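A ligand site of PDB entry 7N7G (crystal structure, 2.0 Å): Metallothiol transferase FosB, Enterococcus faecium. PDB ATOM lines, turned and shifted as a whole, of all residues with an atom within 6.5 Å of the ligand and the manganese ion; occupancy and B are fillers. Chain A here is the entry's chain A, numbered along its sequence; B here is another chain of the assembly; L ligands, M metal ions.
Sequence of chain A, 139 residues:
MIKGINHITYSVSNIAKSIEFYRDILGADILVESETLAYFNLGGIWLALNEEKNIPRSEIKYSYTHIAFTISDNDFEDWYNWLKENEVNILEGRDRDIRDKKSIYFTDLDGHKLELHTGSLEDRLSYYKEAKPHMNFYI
OH of Tyr 105 touches the manganese ion (3.97 Å). Of the 22 residues printed, 4 come within 4 Å of the manganese ion.
The backbone NH of Glu 115 sits at hydrogen-bond distance from the backbone carbonyl oxygen of Ile 67, at 3.0 Å. NE of Arg 124 lies within salt-bridge range of OD1 of Asp 100 (3.7 Å). The side-chain hydroxyl of Tyr 39 of chain B lies within hydrogen-bond range of the side-chain hydroxyl of Tyr 128, at 3.2 Å. The backbone carbonyl oxygen of His 66 is in hydrogen-bond range of the backbone NH of Thr 9 of chain B, at 2.9 Å. The side-chain carboxylate (OD1) of Asp 100 is in salt-bridge range of the guanidinium group (NH2) of Arg 94 (3.2 Å). The backbone carbonyl oxygen (O) of His 7 of chain B lies within hydrogen-bond range of the backbone NH (N) of Ala 68. The side-chain hydroxyl (OH) of Tyr 39 of chain B sits at hydrogen-bond distance from the guanidinium group (NH1) of Arg 124, 3.1 Å away. ND1 of His 66 sits at hydrogen-bond distance from O of Tyr 64, at 2.6 Å.
Tyr 39 of chain B touches the ligand. Trp 46 of chain B touches the ligand. CB of Ala 48 of chain B touches C2 of the ligand, 3.96 Å away. Hydrophobic or aromatic side chains that line the ligand: Tyr 64, His 66, Tyr 105, His 7 of chain B, Tyr 39 of chain B, Trp 46 of chain B and Ala 48 of chain B. Within 4 Å of the ligand: Tyr 64, His 66, Arg 94, Tyr 105, Glu 115, Arg 124, His 7 of chain B, Thr 9 of chain B, Tyr 39 of chain B, Trp 46 of chain B and Ala 48 of chain B.
NH1 of Arg 124 lies within salt-bridge range of O2 of the ligand (2.8 Å). The guanidinium group (NE) of Arg 94 is in salt-bridge range of an oxygen (O4) of the ligand (2.6 Å). An oxygen (O4) of the ligand lies within hydrogen-bond range of the side-chain hydroxyl (OH) of Tyr 64 (2.6 Å). The side-chain hydroxyl of Thr 9 of chain B sits close to an oxygen (O1) of the ligand. OH of Tyr 105 sits close to O3 of the ligand (2.4 Å).
The manganese ion is bound by OE1 of Glu 115 (1.9 Å), O3 of the ligand (2.1 Å), NE2 of His 7 of chain B (2.2 Å), O1 of the ligand (2.3 Å) and NE2 of His 66 (2.3 Å). The manganese ion has five donor atoms within binding distance.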
ATOM      1  N   TYR A  64      -4.984 -12.151 -13.996  1.00  0.00           N
ATOM      2  CA  TYR A  64      -4.026 -13.003 -13.223  1.00  0.00           C
ATOM      3  C   TYR A  64      -3.552 -14.172 -14.101  1.00  0.00           C
ATOM      4  O   TYR A  64      -2.682 -14.936 -13.666  1.00  0.00           O
ATOM      5  CB  TYR A  64      -4.664 -13.520 -11.934  1.00  0.00           C
ATOM      6  CG  TYR A  64      -3.672 -14.031 -10.910  1.00  0.00           C
ATOM      7  CD1 TYR A  64      -2.651 -13.212 -10.480  1.00  0.00           C
ATOM      8  CD2 TYR A  64      -3.751 -15.315 -10.383  1.00  0.00           C
ATOM      9  CE1 TYR A  64      -1.722 -13.650  -9.553  1.00  0.00           C
ATOM     10  CE2 TYR A  64      -2.831 -15.766  -9.439  1.00  0.00           C
ATOM     11  CZ  TYR A  64      -1.811 -14.927  -9.032  1.00  0.00           C
ATOM     12  OH  TYR A  64      -0.875 -15.265  -8.102  1.00  0.00           O
ATOM     13  N   HIS A  66      -1.472 -16.533 -16.177  1.00  0.00           N
ATOM     14  CA  HIS A  66      -0.008 -16.651 -16.329  1.00  0.00           C
ATOM     15  C   HIS A  66       0.411 -18.115 -16.480  1.00  0.00           C
ATOM     16  O   HIS A  66      -0.384 -19.009 -16.207  1.00  0.00           O
ATOM     17  CB  HIS A  66       0.691 -15.990 -15.129  1.00  0.00           C
ATOM     18  CG  HIS A  66       0.458 -16.709 -13.864  1.00  0.00           C
ATOM     19  ND1 HIS A  66      -0.679 -16.526 -13.126  1.00  0.00           N
ATOM     20  CD2 HIS A  66       1.222 -17.620 -13.211  1.00  0.00           C
ATOM     21  CE1 HIS A  66      -0.622 -17.276 -12.041  1.00  0.00           C
ATOM     22  NE2 HIS A  66       0.541 -17.948 -12.078  1.00  0.00           N
ATOM     23  N   ILE A  67       1.655 -18.314 -16.882  1.00  0.00           N
ATOM     24  CA  ILE A  67       2.319 -19.639 -16.983  1.00  0.00           C
ATOM     25  C   ILE A  67       3.526 -19.642 -16.035  1.00  0.00           C
ATOM     26  O   ILE A  67       4.308 -18.665 -16.013  1.00  0.00           O
ATOM     27  CB  ILE A  67       2.714 -19.956 -18.439  1.00  0.00           C
ATOM     28  CG1 ILE A  67       1.522 -19.882 -19.397  1.00  0.00           C
ATOM     29  CG2 ILE A  67       3.374 -21.328 -18.526  1.00  0.00           C
ATOM     30  CD1 ILE A  67       1.833 -20.301 -20.801  1.00  0.00           C
ATOM     31  N   ALA A  68       3.675 -20.694 -15.238  1.00  0.00           N
ATOM     32  CA  ALA A  68       4.778 -20.844 -14.281  1.00  0.00           C
ATOM     33  C   ALA A  68       5.745 -21.929 -14.778  1.00  0.00           C
ATOM     34  O   ALA A  68       5.272 -22.932 -15.241  1.00  0.00           O
ATOM     35  CB  ALA A  68       4.236 -21.161 -12.935  1.00  0.00           C
ATOM     36  N   ARG A  94       1.710 -11.861  -4.710  1.00  0.00           N
ATOM     37  CA  ARG A  94       0.704 -11.964  -3.621  1.00  0.00           C
ATOM     38  C   ARG A  94       1.474 -12.227  -2.316  1.00  0.00           C
ATOM     39  O   ARG A  94       2.665 -12.584  -2.413  1.00  0.00           O
ATOM     40  CB  ARG A  94      -0.361 -13.023  -3.931  1.00  0.00           C
ATOM     41  CG  ARG A  94       0.148 -14.437  -4.167  1.00  0.00           C
ATOM     42  CD  ARG A  94      -0.988 -15.445  -4.362  1.00  0.00           C
ATOM     43  NE  ARG A  94      -0.477 -16.793  -4.548  1.00  0.00           N
ATOM     44  CZ  ARG A  94       0.055 -17.553  -3.594  1.00  0.00           C
ATOM     45  NH1 ARG A  94       0.128 -17.124  -2.337  1.00  0.00           N
ATOM     46  NH2 ARG A  94       0.514 -18.758  -3.896  1.00  0.00           N
ATOM     47  N   ARG A  96       2.635 -14.505   0.802  1.00  0.00           N
ATOM     48  CA  ARG A  96       3.124 -15.903   0.715  1.00  0.00           C
ATOM     49  C   ARG A  96       3.494 -16.493   2.092  1.00  0.00           C
ATOM     50  O   ARG A  96       4.549 -16.105   2.649  1.00  0.00           O
ATOM     51  CB  ARG A  96       4.367 -16.018  -0.160  1.00  0.00           C
ATOM     52  CG  ARG A  96       4.145 -15.771  -1.638  1.00  0.00           C
ATOM     53  CD  ARG A  96       5.305 -16.305  -2.445  1.00  0.00           C
ATOM     54  NE  ARG A  96       5.041 -17.660  -2.904  1.00  0.00           N
ATOM     55  CZ  ARG A  96       4.242 -17.989  -3.925  1.00  0.00           C
ATOM     56  NH1 ARG A  96       3.592 -17.061  -4.618  1.00  0.00           N
ATOM     57  NH2 ARG A  96       4.093 -19.260  -4.253  1.00  0.00           N
ATOM     58  N   ASP A 100       3.626 -22.020   0.857  1.00  0.00           N
ATOM     59  CA  ASP A 100       3.288 -21.767  -0.571  1.00  0.00           C
ATOM     60  C   ASP A 100       4.503 -22.010  -1.460  1.00  0.00           C
ATOM     61  O   ASP A 100       4.379 -21.803  -2.640  1.00  0.00           O
ATOM     62  CB  ASP A 100       3.040 -20.290  -0.845  1.00  0.00           C
ATOM     63  CG  ASP A 100       1.607 -19.861  -0.689  1.00  0.00           C
ATOM     64  OD1 ASP A 100       0.750 -20.530  -1.274  1.00  0.00           O
ATOM     65  OD2 ASP A 100       1.359 -18.869   0.034  1.00  0.00           O
ATOM     66  N   SER A 103       8.235 -17.958  -5.289  1.00  0.00           N
ATOM     67  CA  SER A 103       7.856 -17.517  -6.654  1.00  0.00           C
ATOM     68  C   SER A 103       8.418 -16.131  -6.971  1.00  0.00           C
ATOM     69  O   SER A 103       8.490 -15.320  -6.094  1.00  0.00           O
ATOM     70  CB  SER A 103       6.376 -17.431  -6.820  1.00  0.00           C
ATOM     71  OG  SER A 103       5.725 -18.667  -6.745  1.00  0.00           O
ATOM     72  N   TYR A 105       7.348 -13.393  -9.966  1.00  0.00           N
ATOM     73  CA  TYR A 105       6.385 -13.028 -11.051  1.00  0.00           C
ATOM     74  C   TYR A 105       6.981 -11.894 -11.883  1.00  0.00           C
ATOM     75  O   TYR A 105       7.546 -10.936 -11.327  1.00  0.00           O
ATOM     76  CB  TYR A 105       5.035 -12.638 -10.470  1.00  0.00           C
ATOM     77  CG  TYR A 105       4.365 -13.744  -9.672  1.00  0.00           C
ATOM     78  CD1 TYR A 105       4.619 -13.908  -8.322  1.00  0.00           C
ATOM     79  CD2 TYR A 105       3.487 -14.627 -10.281  1.00  0.00           C
ATOM     80  CE1 TYR A 105       4.010 -14.927  -7.588  1.00  0.00           C
ATOM     81  CE2 TYR A 105       2.882 -15.648  -9.570  1.00  0.00           C
ATOM     82  CZ  TYR A 105       3.135 -15.803  -8.209  1.00  0.00           C
ATOM     83  OH  TYR A 105       2.530 -16.810  -7.499  1.00  0.00           O
ATOM     84  N   GLU A 115       5.939 -16.765 -14.278  1.00  0.00           N
ATOM     85  CA  GLU A 115       6.280 -17.163 -12.899  1.00  0.00           C
ATOM     86  C   GLU A 115       7.437 -18.145 -12.916  1.00  0.00           C
ATOM     87  O   GLU A 115       7.406 -19.108 -13.716  1.00  0.00           O
ATOM     88  CB  GLU A 115       5.049 -17.717 -12.190  1.00  0.00           C
ATOM     89  CG  GLU A 115       5.269 -17.886 -10.705  1.00  0.00           C
ATOM     90  CD  GLU A 115       4.179 -18.687 -10.034  1.00  0.00           C
ATOM     91  OE1 GLU A 115       3.112 -18.830 -10.664  1.00  0.00           O
ATOM     92  OE2 GLU A 115       4.404 -19.205  -8.926  1.00  0.00           O
ATOM     93  N   HIS A 117       8.716 -20.652 -10.122  1.00  0.00           N
ATOM     94  CA  HIS A 117       8.163 -21.289  -8.908  1.00  0.00           C
ATOM     95  C   HIS A 117       9.017 -22.494  -8.498  1.00  0.00           C
ATOM     96  O   HIS A 117       9.381 -23.301  -9.401  1.00  0.00           O
ATOM     97  CB  HIS A 117       6.712 -21.714  -9.181  1.00  0.00           C
ATOM     98  CG  HIS A 117       6.024 -22.199  -7.959  1.00  0.00           C
ATOM     99  ND1 HIS A 117       6.049 -21.475  -6.773  1.00  0.00           N
ATOM    100  CD2 HIS A 117       5.381 -23.366  -7.695  1.00  0.00           C
ATOM    101  CE1 HIS A 117       5.368 -22.155  -5.851  1.00  0.00           C
ATOM    102  NE2 HIS A 117       4.945 -23.320  -6.392  1.00  0.00           N
ATOM    103  N   ARG A 124       1.609 -27.877  -2.929  1.00  0.00           N
ATOM    104  CA  ARG A 124       0.451 -26.971  -2.765  1.00  0.00           C
ATOM    105  C   ARG A 124      -0.722 -27.730  -2.148  1.00  0.00           C
ATOM    106  O   ARG A 124      -1.374 -27.180  -1.258  1.00  0.00           O
ATOM    107  CB  ARG A 124       0.036 -26.356  -4.091  1.00  0.00           C
ATOM    108  CG  ARG A 124      -0.995 -25.240  -3.939  1.00  0.00           C
ATOM    109  CD  ARG A 124      -0.600 -24.083  -3.068  1.00  0.00           C
ATOM    110  NE  ARG A 124       0.655 -23.489  -3.461  1.00  0.00           N
ATOM    111  CZ  ARG A 124       0.791 -22.528  -4.389  1.00  0.00           C
ATOM    112  NH1 ARG A 124      -0.269 -22.019  -5.002  1.00  0.00           N
ATOM    113  NH2 ARG A 124       1.982 -22.045  -4.650  1.00  0.00           N
ATOM    114  N   TYR A 128      -2.444 -26.830   1.321  1.00  0.00           N
ATOM    115  CA  TYR A 128      -3.871 -26.428   1.367  1.00  0.00           C
ATOM    116  C   TYR A 128      -4.661 -27.384   2.264  1.00  0.00           C
ATOM    117  O   TYR A 128      -5.582 -26.912   2.937  1.00  0.00           O
ATOM    118  CB  TYR A 128      -4.444 -26.382  -0.046  1.00  0.00           C
ATOM    119  CG  TYR A 128      -4.132 -25.132  -0.815  1.00  0.00           C
ATOM    120  CD1 TYR A 128      -3.403 -24.092  -0.248  1.00  0.00           C
ATOM    121  CD2 TYR A 128      -4.606 -24.959  -2.103  1.00  0.00           C
ATOM    122  CE1 TYR A 128      -3.145 -22.928  -0.934  1.00  0.00           C
ATOM    123  CE2 TYR A 128      -4.344 -23.789  -2.802  1.00  0.00           C
ATOM    124  CZ  TYR A 128      -3.632 -22.769  -2.216  1.00  0.00           C
ATOM    125  OH  TYR A 128      -3.384 -21.626  -2.908  1.00  0.00           O
ATOM    126  N   HIS B   7       3.061 -24.889 -13.933  1.00  0.00           N
ATOM    127  CA  HIS B   7       1.576 -24.807 -13.933  1.00  0.00           C
ATOM    128  C   HIS B   7       1.097 -23.751 -14.904  1.00  0.00           C
ATOM    129  O   HIS B   7       1.892 -22.863 -15.286  1.00  0.00           O
ATOM    130  CB  HIS B   7       0.982 -24.609 -12.515  1.00  0.00           C
ATOM    131  CG  HIS B   7       1.362 -23.361 -11.795  1.00  0.00           C
ATOM    132  ND1 HIS B   7       2.498 -23.272 -10.985  1.00  0.00           N
ATOM    133  CD2 HIS B   7       0.707 -22.177 -11.658  1.00  0.00           C
ATOM    134  CE1 HIS B   7       2.537 -22.071 -10.441  1.00  0.00           C
ATOM    135  NE2 HIS B   7       1.463 -21.385 -10.838  1.00  0.00           N
ATOM    136  N   ILE B   8      -0.172 -23.881 -15.271  1.00  0.00           N
ATOM    137  CA  ILE B   8      -0.889 -22.935 -16.154  1.00  0.00           C
ATOM    138  C   ILE B   8      -2.055 -22.393 -15.345  1.00  0.00           C
ATOM    139  O   ILE B   8      -2.802 -23.201 -14.791  1.00  0.00           O
ATOM    140  CB  ILE B   8      -1.329 -23.580 -17.469  1.00  0.00           C
ATOM    141  CG1 ILE B   8      -0.140 -24.067 -18.302  1.00  0.00           C
ATOM    142  CG2 ILE B   8      -2.192 -22.611 -18.267  1.00  0.00           C
ATOM    143  CD1 ILE B   8      -0.577 -24.922 -19.465  1.00  0.00           C
ATOM    144  N   THR B   9      -2.127 -21.067 -15.230  1.00  0.00           N
ATOM    145  CA  THR B   9      -3.213 -20.396 -14.484  1.00  0.00           C
ATOM    146  C   THR B   9      -4.059 -19.558 -15.458  1.00  0.00           C
ATOM    147  O   THR B   9      -3.512 -18.683 -16.124  1.00  0.00           O
ATOM    148  CB  THR B   9      -2.659 -19.578 -13.315  1.00  0.00           C
ATOM    149  OG1 THR B   9      -2.028 -20.463 -12.387  1.00  0.00           O
ATOM    150  CG2 THR B   9      -3.753 -18.837 -12.592  1.00  0.00           C
ATOM    151  N   LEU B  37     -11.064 -20.508  -6.537  1.00  0.00           N
ATOM    152  CA  LEU B  37      -9.992 -21.235  -7.274  1.00  0.00           C
ATOM    153  C   LEU B  37     -10.289 -22.711  -7.406  1.00  0.00           C
ATOM    154  O   LEU B  37     -11.030 -23.263  -6.617  1.00  0.00           O
ATOM    155  CB  LEU B  37      -8.608 -20.979  -6.657  1.00  0.00           C
ATOM    156  CG  LEU B  37      -8.103 -21.804  -5.491  1.00  0.00           C
ATOM    157  CD1 LEU B  37      -7.979 -23.293  -5.807  1.00  0.00           C
ATOM    158  CD2 LEU B  37      -6.724 -21.292  -5.093  1.00  0.00           C
ATOM    159  N   TYR B  39      -7.995 -26.363  -8.863  1.00  0.00           N
ATOM    160  CA  TYR B  39      -6.826 -27.029  -9.492  1.00  0.00           C
ATOM    161  C   TYR B  39      -7.260 -28.342 -10.152  1.00  0.00           C
ATOM    162  O   TYR B  39      -8.121 -29.062  -9.586  1.00  0.00           O
ATOM    163  CB  TYR B  39      -5.730 -27.352  -8.479  1.00  0.00           C
ATOM    164  CG  TYR B  39      -5.071 -26.176  -7.801  1.00  0.00           C
ATOM    165  CD1 TYR B  39      -5.094 -24.889  -8.317  1.00  0.00           C
ATOM    166  CD2 TYR B  39      -4.368 -26.374  -6.623  1.00  0.00           C
ATOM    167  CE1 TYR B  39      -4.447 -23.836  -7.671  1.00  0.00           C
ATOM    168  CE2 TYR B  39      -3.749 -25.326  -5.954  1.00  0.00           C
ATOM    169  CZ  TYR B  39      -3.777 -24.054  -6.477  1.00  0.00           C
ATOM    170  OH  TYR B  39      -3.108 -23.048  -5.795  1.00  0.00           O
ATOM    171  N   TRP B  46      -0.458 -29.358 -14.207  1.00  0.00           N
ATOM    172  CA  TRP B  46      -1.157 -28.619 -13.143  1.00  0.00           C
ATOM    173  C   TRP B  46      -1.872 -27.417 -13.767  1.00  0.00           C
ATOM    174  O   TRP B  46      -1.166 -26.466 -14.201  1.00  0.00           O
ATOM    175  CB  TRP B  46      -0.154 -28.220 -12.050  1.00  0.00           C
ATOM    176  CG  TRP B  46      -0.692 -27.375 -10.930  1.00  0.00           C
ATOM    177  CD1 TRP B  46      -1.988 -27.040 -10.665  1.00  0.00           C
ATOM    178  CD2 TRP B  46       0.100 -26.781  -9.865  1.00  0.00           C
ATOM    179  NE1 TRP B  46      -2.060 -26.241  -9.550  1.00  0.00           N
ATOM    180  CE2 TRP B  46      -0.799 -26.073  -9.028  1.00  0.00           C
ATOM    181  CE3 TRP B  46       1.472 -26.771  -9.569  1.00  0.00           C
ATOM    182  CZ2 TRP B  46      -0.352 -25.355  -7.917  1.00  0.00           C
ATOM    183  CZ3 TRP B  46       1.895 -26.074  -8.457  1.00  0.00           C
ATOM    184  CH2 TRP B  46       0.997 -25.382  -7.653  1.00  0.00           C
ATOM    185  N   ALA B  48      -4.721 -24.428 -13.158  1.00  0.00           N
ATOM    186  CA  ALA B  48      -5.379 -23.634 -12.114  1.00  0.00           C
ATOM    187  C   ALA B  48      -6.308 -22.620 -12.765  1.00  0.00           C
ATOM    188  O   ALA B  48      -5.945 -22.039 -13.806  1.00  0.00           O
ATOM    189  CB  ALA B  48      -4.351 -22.999 -11.219  1.00  0.00           C
ATOM    190  N   LEU B  49      -7.469 -22.436 -12.137  1.00  0.00           N
ATOM    191  CA  LEU B  49      -8.434 -21.372 -12.448  1.00  0.00           C
ATOM    192  C   LEU B  49      -8.508 -20.494 -11.205  1.00  0.00           C
ATOM    193  O   LEU B  49      -8.590 -21.078 -10.123  1.00  0.00           O
ATOM    194  CB  LEU B  49      -9.811 -21.964 -12.766  1.00  0.00           C
ATOM    195  CG  LEU B  49      -9.870 -23.122 -13.751  1.00  0.00           C
ATOM    196  CD1 LEU B  49     -11.303 -23.631 -13.885  1.00  0.00           C
ATOM    197  CD2 LEU B  49      -9.323 -22.699 -15.115  1.00  0.00           C
ATOM    198  N   ASN B  50      -8.484 -19.174 -11.404  1.00  0.00           N
ATOM    199  CA  ASN B  50      -8.710 -18.122 -10.387  1.00  0.00           C
ATOM    200  C   ASN B  50      -9.831 -17.201 -10.885  1.00  0.00           C
ATOM    201  O   ASN B  50      -9.685 -16.632 -11.961  1.00  0.00           O
ATOM    202  CB  ASN B  50      -7.434 -17.318 -10.112  1.00  0.00           C
ATOM    203  CG  ASN B  50      -6.409 -18.191  -9.433  1.00  0.00           C
ATOM    204  OD1 ASN B  50      -5.747 -18.997 -10.096  1.00  0.00           O
ATOM    205  ND2 ASN B  50      -6.352 -18.133  -8.118  1.00  0.00           N
HETATM  206  C1  LIG L   1      -1.583 -19.176  -8.803  1.00  0.00           C
HETATM  207  C2  LIG L   1      -2.018 -20.497  -9.233  1.00  0.00           C
HETATM  208  C3  LIG L   1      -1.642 -21.635  -8.366  1.00  0.00           C
HETATM  209  O1  LIG L   1      -0.948 -19.791  -9.955  1.00  0.00           O
HETATM  210  P1  LIG L   1      -0.303 -18.770  -7.624  1.00  0.00           P
HETATM  211  O2  LIG L   1       0.139 -19.772  -6.585  1.00  0.00           O
HETATM  212  O3  LIG L   1       0.866 -18.260  -8.489  1.00  0.00           O
HETATM  213  O4  LIG L   1      -1.067 -17.644  -6.966  1.00  0.00           O
HETATM  214 MN    MN M   1       1.242 -19.266 -10.338  1.00  0.00          MN
